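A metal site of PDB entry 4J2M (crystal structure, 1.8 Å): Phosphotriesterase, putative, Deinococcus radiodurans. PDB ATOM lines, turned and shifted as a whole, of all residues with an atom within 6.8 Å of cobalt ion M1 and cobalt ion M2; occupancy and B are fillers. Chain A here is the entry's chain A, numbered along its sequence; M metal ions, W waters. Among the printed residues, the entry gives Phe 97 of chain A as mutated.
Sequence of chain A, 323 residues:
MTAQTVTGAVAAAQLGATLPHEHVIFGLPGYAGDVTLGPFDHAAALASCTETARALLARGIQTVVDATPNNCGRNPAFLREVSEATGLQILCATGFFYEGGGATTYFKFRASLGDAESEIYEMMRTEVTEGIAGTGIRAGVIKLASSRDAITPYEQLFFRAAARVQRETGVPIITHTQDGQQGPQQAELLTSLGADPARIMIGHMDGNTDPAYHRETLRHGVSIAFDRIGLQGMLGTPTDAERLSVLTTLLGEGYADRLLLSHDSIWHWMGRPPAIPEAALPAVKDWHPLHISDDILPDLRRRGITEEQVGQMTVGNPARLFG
Cobalt ion M2 is bound by water W1, a ring nitrogen (NE2) of His 23, OQ1 of KCX 143, a ring nitrogen (NE2) of His 21 and the side-chain carboxylate of Asp 264.
Cobalt ion M2 has five donor atoms within binding distance.
Of the 19 residues printed, 3 come within 4 Å of cobalt ion M1.
Along chain A the residues within 4 Å of cobalt ion M1 span positions 143 to 204.
The nearest printed residue that does not touch cobalt ion M1 is Asp 264 (4.1 Å).
Cobalt ion M1 is bound by OQ2 of KCX 143, at 1.9 Å.
NE2 of His 204 binds cobalt ion M1, 2.1 Å away.
Cobalt ion M1 is bound by water W1.
ND1 of His 176 binds cobalt ion M1.
Cobalt ion M1 has four donor atoms within binding distance.
The backbone carbonyl oxygen of His 204 is in hydrogen-bond range of the side-chain hydroxyl of Thr 177, at 3.3 Å.
OD2 of Asp 264 lies within salt-bridge range of NE of Arg 228 (2.9 Å).
The backbone carbonyl oxygen of Ala 67 is in hydrogen-bond range of NZ of KCX 143, at 3.0 Å.
N of Asp 264 lies within hydrogen-bond range of OE1 of Glu 22, 3.4 Å away.
ND1 of His 204 lies within hydrogen-bond range of OD1 of Asp 227 (2.7 Å).
The backbone NH (N) of His 23 sits at hydrogen-bond distance from the backbone carbonyl oxygen (O) of Ser 265, at 2.8 Å.
The backbone carbonyl oxygen of Asp 227 is in hydrogen-bond range of the backbone NH of Asp 264 (2.9 Å).
The side-chain amide oxygen of Gln 178 sits at hydrogen-bond distance from a ring nitrogen (NE2) of His 176.
Within 4 Å of cobalt ion M2: His 21, His 23, KCX 143 and Asp 264.
The nearest printed residue that does not touch cobalt ion M2 is His 204 (4.2 Å).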
ATOM      1  N   HIS A  21     -28.359  14.836 -30.457  1.00  0.00           N
ATOM      2  CA  HIS A  21     -28.633  16.225 -30.064  1.00  0.00           C
ATOM      3  C   HIS A  21     -29.501  16.889 -31.152  1.00  0.00           C
ATOM      4  O   HIS A  21     -28.990  17.363 -32.163  1.00  0.00           O
ATOM      5  CB  HIS A  21     -27.365  17.037 -29.871  1.00  0.00           C
ATOM      6  CG  HIS A  21     -27.601  18.423 -29.313  1.00  0.00           C
ATOM      7  ND1 HIS A  21     -27.012  18.872 -28.147  1.00  0.00           N
ATOM      8  CD2 HIS A  21     -28.394  19.428 -29.753  1.00  0.00           C
ATOM      9  CE1 HIS A  21     -27.409  20.120 -27.909  1.00  0.00           C
ATOM     10  NE2 HIS A  21     -28.245  20.481 -28.861  1.00  0.00           N
ATOM     11  N   GLU A  22     -30.798  16.912 -30.889  1.00  0.00           N
ATOM     12  CA  GLU A  22     -31.771  17.571 -31.771  1.00  0.00           C
ATOM     13  C   GLU A  22     -32.862  18.233 -30.925  1.00  0.00           C
ATOM     14  O   GLU A  22     -32.984  18.009 -29.715  1.00  0.00           O
ATOM     15  CB  GLU A  22     -32.441  16.555 -32.709  1.00  0.00           C
ATOM     16  CG  GLU A  22     -31.489  15.603 -33.444  1.00  0.00           C
ATOM     17  CD  GLU A  22     -30.687  16.300 -34.533  1.00  0.00           C
ATOM     18  OE1 GLU A  22     -31.161  17.366 -35.034  1.00  0.00           O
ATOM     19  OE2 GLU A  22     -29.600  15.789 -34.892  1.00  0.00           O
ATOM     20  N   HIS A  23     -33.688  19.036 -31.593  1.00  0.00           N
ATOM     21  CA  HIS A  23     -34.798  19.677 -30.918  1.00  0.00           C
ATOM     22  C   HIS A  23     -36.100  19.431 -31.692  1.00  0.00           C
ATOM     23  O   HIS A  23     -36.318  20.003 -32.761  1.00  0.00           O
ATOM     24  CB  HIS A  23     -34.487  21.171 -30.776  1.00  0.00           C
ATOM     25  CG  HIS A  23     -33.251  21.470 -29.978  1.00  0.00           C
ATOM     26  ND1 HIS A  23     -33.242  21.435 -28.598  1.00  0.00           N
ATOM     27  CD2 HIS A  23     -31.991  21.820 -30.349  1.00  0.00           C
ATOM     28  CE1 HIS A  23     -32.033  21.726 -28.147  1.00  0.00           C
ATOM     29  NE2 HIS A  23     -31.258  21.976 -29.191  1.00  0.00           N
ATOM     30  N   PHE A  26     -38.697  23.819 -30.095  1.00  0.00           N
ATOM     31  CA  PHE A  26     -37.745  24.701 -29.441  1.00  0.00           C
ATOM     32  C   PHE A  26     -38.214  26.118 -29.498  1.00  0.00           C
ATOM     33  O   PHE A  26     -38.545  26.607 -30.578  1.00  0.00           O
ATOM     34  CB  PHE A  26     -36.392  24.653 -30.136  1.00  0.00           C
ATOM     35  CG  PHE A  26     -35.282  25.365 -29.405  1.00  0.00           C
ATOM     36  CD1 PHE A  26     -34.505  24.691 -28.466  1.00  0.00           C
ATOM     37  CD2 PHE A  26     -35.004  26.690 -29.668  1.00  0.00           C
ATOM     38  CE1 PHE A  26     -33.472  25.352 -27.783  1.00  0.00           C
ATOM     39  CE2 PHE A  26     -33.966  27.351 -29.003  1.00  0.00           C
ATOM     40  CZ  PHE A  26     -33.207  26.672 -28.050  1.00  0.00           C
ATOM     41  N   ALA A  67     -32.455  17.593 -26.755  1.00  0.00           N
ATOM     42  CA  ALA A  67     -31.576  18.292 -25.832  1.00  0.00           C
ATOM     43  C   ALA A  67     -32.191  19.593 -25.312  1.00  0.00           C
ATOM     44  O   ALA A  67     -31.490  20.408 -24.734  1.00  0.00           O
ATOM     45  CB  ALA A  67     -30.316  18.594 -26.525  1.00  0.00           C
ATOM     46  N   THR A  68     -33.495  19.767 -25.505  1.00  0.00           N
ATOM     47  CA  THR A  68     -34.168  21.047 -25.190  1.00  0.00           C
ATOM     48  C   THR A  68     -34.179  21.355 -23.688  1.00  0.00           C
ATOM     49  O   THR A  68     -34.813  20.634 -22.914  1.00  0.00           O
ATOM     50  CB  THR A  68     -35.622  21.046 -25.719  1.00  0.00           C
ATOM     51  OG1 THR A  68     -35.620  20.735 -27.122  1.00  0.00           O
ATOM     52  CG2 THR A  68     -36.286  22.413 -25.515  1.00  0.00           C
ATOM     53  N   PRO A  69     -33.527  22.454 -23.274  1.00  0.00           N
ATOM     54  CA  PRO A  69     -33.553  22.781 -21.836  1.00  0.00           C
ATOM     55  C   PRO A  69     -34.947  23.205 -21.298  1.00  0.00           C
ATOM     56  O   PRO A  69     -35.828  23.589 -22.076  1.00  0.00           O
ATOM     57  CB  PRO A  69     -32.549  23.942 -21.708  1.00  0.00           C
ATOM     58  CG  PRO A  69     -31.771  23.954 -22.975  1.00  0.00           C
ATOM     59  CD  PRO A  69     -32.695  23.395 -24.035  1.00  0.00           C
ATOM     60  N   PHE A  97     -30.435  26.655 -19.707  1.00  0.00           N
ATOM     61  CA  PHE A  97     -29.492  27.080 -20.733  1.00  0.00           C
ATOM     62  C   PHE A  97     -28.433  28.188 -20.304  1.00  0.00           C
ATOM     63  O   PHE A  97     -28.716  28.955 -19.383  1.00  0.00           O
ATOM     64  CB  PHE A  97     -30.359  27.475 -21.955  1.00  0.00           C
ATOM     65  CG  PHE A  97     -29.644  28.288 -22.888  1.00  0.00           C
ATOM     66  CD1 PHE A  97     -28.385  27.927 -23.145  1.00  0.00           C
ATOM     67  CD2 PHE A  97     -30.181  29.389 -23.501  1.00  0.00           C
ATOM     68  CE1 PHE A  97     -27.618  28.614 -23.956  1.00  0.00           C
ATOM     69  CE2 PHE A  97     -29.417  30.128 -24.355  1.00  0.00           C
ATOM     70  CZ  PHE A  97     -28.119  29.731 -24.584  1.00  0.00           C
ATOM     71  N   KCX A 143     -28.856  18.188 -19.404  1.00  0.00           N
ATOM     72  CA  KCX A 143     -28.394  19.232 -20.285  1.00  0.00           C
ATOM     73  CB  KCX A 143     -29.544  19.844 -21.105  1.00  0.00           C
ATOM     74  CG  KCX A 143     -29.176  20.138 -22.563  1.00  0.00           C
ATOM     75  CD  KCX A 143     -28.034  21.114 -22.684  1.00  0.00           C
ATOM     76  CE  KCX A 143     -27.658  21.485 -24.111  1.00  0.00           C
ATOM     77  NZ  KCX A 143     -28.796  21.792 -25.081  1.00  0.00           N
ATOM     78  C   KCX A 143     -27.660  20.315 -19.522  1.00  0.00           C
ATOM     79  O   KCX A 143     -28.239  20.978 -18.658  1.00  0.00           O
ATOM     80  CX  KCX A 143     -28.649  22.518 -26.195  1.00  0.00           C
ATOM     81  OQ1 KCX A 143     -29.639  22.625 -26.939  1.00  0.00           O
ATOM     82  OQ2 KCX A 143     -27.592  23.075 -26.495  1.00  0.00           O
ATOM     83  N   ALA A 145     -24.912  23.828 -20.031  1.00  0.00           N
ATOM     84  CA  ALA A 145     -24.457  24.803 -20.996  1.00  0.00           C
ATOM     85  C   ALA A 145     -23.539  25.797 -20.323  1.00  0.00           C
ATOM     86  O   ALA A 145     -23.737  26.122 -19.161  1.00  0.00           O
ATOM     87  CB  ALA A 145     -25.648  25.516 -21.595  1.00  0.00           C
ATOM     88  N   THR A 175     -23.818  18.406 -23.262  1.00  0.00           N
ATOM     89  CA  THR A 175     -23.590  19.818 -23.062  1.00  0.00           C
ATOM     90  C   THR A 175     -23.695  20.671 -24.313  1.00  0.00           C
ATOM     91  O   THR A 175     -23.640  20.159 -25.451  1.00  0.00           O
ATOM     92  CB  THR A 175     -22.185  20.118 -22.471  1.00  0.00           C
ATOM     93  OG1 THR A 175     -21.204  20.143 -23.513  1.00  0.00           O
ATOM     94  CG2 THR A 175     -21.824  19.103 -21.421  1.00  0.00           C
ATOM     95  N   HIS A 176     -23.840  21.980 -24.053  1.00  0.00           N
ATOM     96  CA  HIS A 176     -23.722  23.057 -25.023  1.00  0.00           C
ATOM     97  C   HIS A 176     -22.421  23.819 -24.786  1.00  0.00           C
ATOM     98  O   HIS A 176     -22.161  24.255 -23.662  1.00  0.00           O
ATOM     99  CB  HIS A 176     -24.929  24.006 -24.824  1.00  0.00           C
ATOM    100  CG  HIS A 176     -24.839  25.301 -25.564  1.00  0.00           C
ATOM    101  ND1 HIS A 176     -25.662  25.593 -26.643  1.00  0.00           N
ATOM    102  CD2 HIS A 176     -24.089  26.406 -25.364  1.00  0.00           C
ATOM    103  CE1 HIS A 176     -25.394  26.803 -27.087  1.00  0.00           C
ATOM    104  NE2 HIS A 176     -24.439  27.324 -26.334  1.00  0.00           N
ATOM    105  N   THR A 177     -21.623  24.022 -25.816  1.00  0.00           N
ATOM    106  CA  THR A 177     -20.499  24.944 -25.721  1.00  0.00           C
ATOM    107  C   THR A 177     -20.808  26.084 -26.652  1.00  0.00           C
ATOM    108  O   THR A 177     -21.393  25.867 -27.707  1.00  0.00           O
ATOM    109  CB  THR A 177     -19.107  24.330 -26.103  1.00  0.00           C
ATOM    110  OG1 THR A 177     -19.111  23.826 -27.452  1.00  0.00           O
ATOM    111  CG2 THR A 177     -18.691  23.251 -25.109  1.00  0.00           C
ATOM    112  N   GLN A 178     -20.399  27.291 -26.255  1.00  0.00           N
ATOM    113  CA  GLN A 178     -20.704  28.524 -26.977  1.00  0.00           C
ATOM    114  C   GLN A 178     -19.496  28.960 -27.804  1.00  0.00           C
ATOM    115  O   GLN A 178     -18.401  29.086 -27.255  1.00  0.00           O
ATOM    116  CB  GLN A 178     -21.069  29.630 -25.961  1.00  0.00           C
ATOM    117  CG  GLN A 178     -21.534  30.942 -26.576  1.00  0.00           C
ATOM    118  CD  GLN A 178     -22.828  30.817 -27.390  1.00  0.00           C
ATOM    119  OE1 GLN A 178     -23.689  29.993 -27.073  1.00  0.00           O
ATOM    120  NE2 GLN A 178     -22.969  31.641 -28.418  1.00  0.00           N
ATOM    121  N   HIS A 204     -21.366  20.622 -29.294  1.00  0.00           N
ATOM    122  CA  HIS A 204     -21.004  21.689 -30.219  1.00  0.00           C
ATOM    123  C   HIS A 204     -19.488  21.809 -30.433  1.00  0.00           C
ATOM    124  O   HIS A 204     -18.956  22.908 -30.628  1.00  0.00           O
ATOM    125  CB  HIS A 204     -21.590  23.052 -29.792  1.00  0.00           C
ATOM    126  CG  HIS A 204     -23.059  23.022 -29.472  1.00  0.00           C
ATOM    127  ND1 HIS A 204     -23.929  22.117 -30.015  1.00  0.00           N
ATOM    128  CD2 HIS A 204     -23.799  23.817 -28.651  1.00  0.00           C
ATOM    129  CE1 HIS A 204     -25.150  22.331 -29.550  1.00  0.00           C
ATOM    130  NE2 HIS A 204     -25.092  23.349 -28.704  1.00  0.00           N
ATOM    131  N   ASP A 227     -22.235  18.278 -33.489  1.00  0.00           N
ATOM    132  CA  ASP A 227     -23.681  18.165 -33.412  1.00  0.00           C
ATOM    133  C   ASP A 227     -24.449  19.357 -34.002  1.00  0.00           C
ATOM    134  O   ASP A 227     -25.652  19.453 -33.794  1.00  0.00           O
ATOM    135  CB  ASP A 227     -24.164  17.867 -31.989  1.00  0.00           C
ATOM    136  CG  ASP A 227     -23.637  18.860 -30.975  1.00  0.00           C
ATOM    137  OD1 ASP A 227     -23.143  19.921 -31.395  1.00  0.00           O
ATOM    138  OD2 ASP A 227     -23.691  18.547 -29.770  1.00  0.00           O
ATOM    139  N   ARG A 228     -23.787  20.195 -34.794  1.00  0.00           N
ATOM    140  CA  ARG A 228     -24.509  21.235 -35.538  1.00  0.00           C
ATOM    141  C   ARG A 228     -24.225  21.099 -37.032  1.00  0.00           C
ATOM    142  O   ARG A 228     -24.148  22.075 -37.773  1.00  0.00           O
ATOM    143  CB  ARG A 228     -24.129  22.622 -35.037  1.00  0.00           C
ATOM    144  CG  ARG A 228     -24.348  22.712 -33.538  1.00  0.00           C
ATOM    145  CD  ARG A 228     -24.032  24.044 -33.005  1.00  0.00           C
ATOM    146  NE  ARG A 228     -25.253  24.825 -32.885  1.00  0.00           N
ATOM    147  CZ  ARG A 228     -25.290  26.047 -32.388  1.00  0.00           C
ATOM    148  NH1 ARG A 228     -24.175  26.617 -31.946  1.00  0.00           N
ATOM    149  NH2 ARG A 228     -26.449  26.692 -32.329  1.00  0.00           N
ATOM    150  N   ASP A 264     -28.496  19.427 -34.358  1.00  0.00           N
ATOM    151  CA  ASP A 264     -29.027  20.505 -33.509  1.00  0.00           C
ATOM    152  C   ASP A 264     -30.179  21.181 -34.265  1.00  0.00           C
ATOM    153  O   ASP A 264     -30.373  22.403 -34.201  1.00  0.00           O
ATOM    154  CB  ASP A 264     -27.942  21.542 -33.193  1.00  0.00           C
ATOM    155  CG  ASP A 264     -28.262  22.405 -31.936  1.00  0.00           C
ATOM    156  OD1 ASP A 264     -29.130  22.054 -31.106  1.00  0.00           O
ATOM    157  OD2 ASP A 264     -27.589  23.443 -31.761  1.00  0.00           O
ATOM    158  N   SER A 265     -30.950  20.373 -34.980  1.00  0.00           N
ATOM    159  CA  SER A 265     -32.038  20.898 -35.813  1.00  0.00           C
ATOM    160  C   SER A 265     -33.256  21.243 -34.949  1.00  0.00           C
ATOM    161  O   SER A 265     -33.397  20.752 -33.830  1.00  0.00           O
ATOM    162  CB  SER A 265     -32.379  19.873 -36.922  1.00  0.00           C
ATOM    163  OG  SER A 265     -32.941  18.704 -36.369  1.00  0.00           O
HETATM  164 CO    CO M   1     -26.748  24.203 -27.815  1.00  0.00          CO
HETATM  165 CO    CO M   2     -29.324  22.301 -29.001  1.00  0.00          CO
HETATM  166  O   HOH W   1     -28.248  23.769 -29.239  1.00  0.00           O
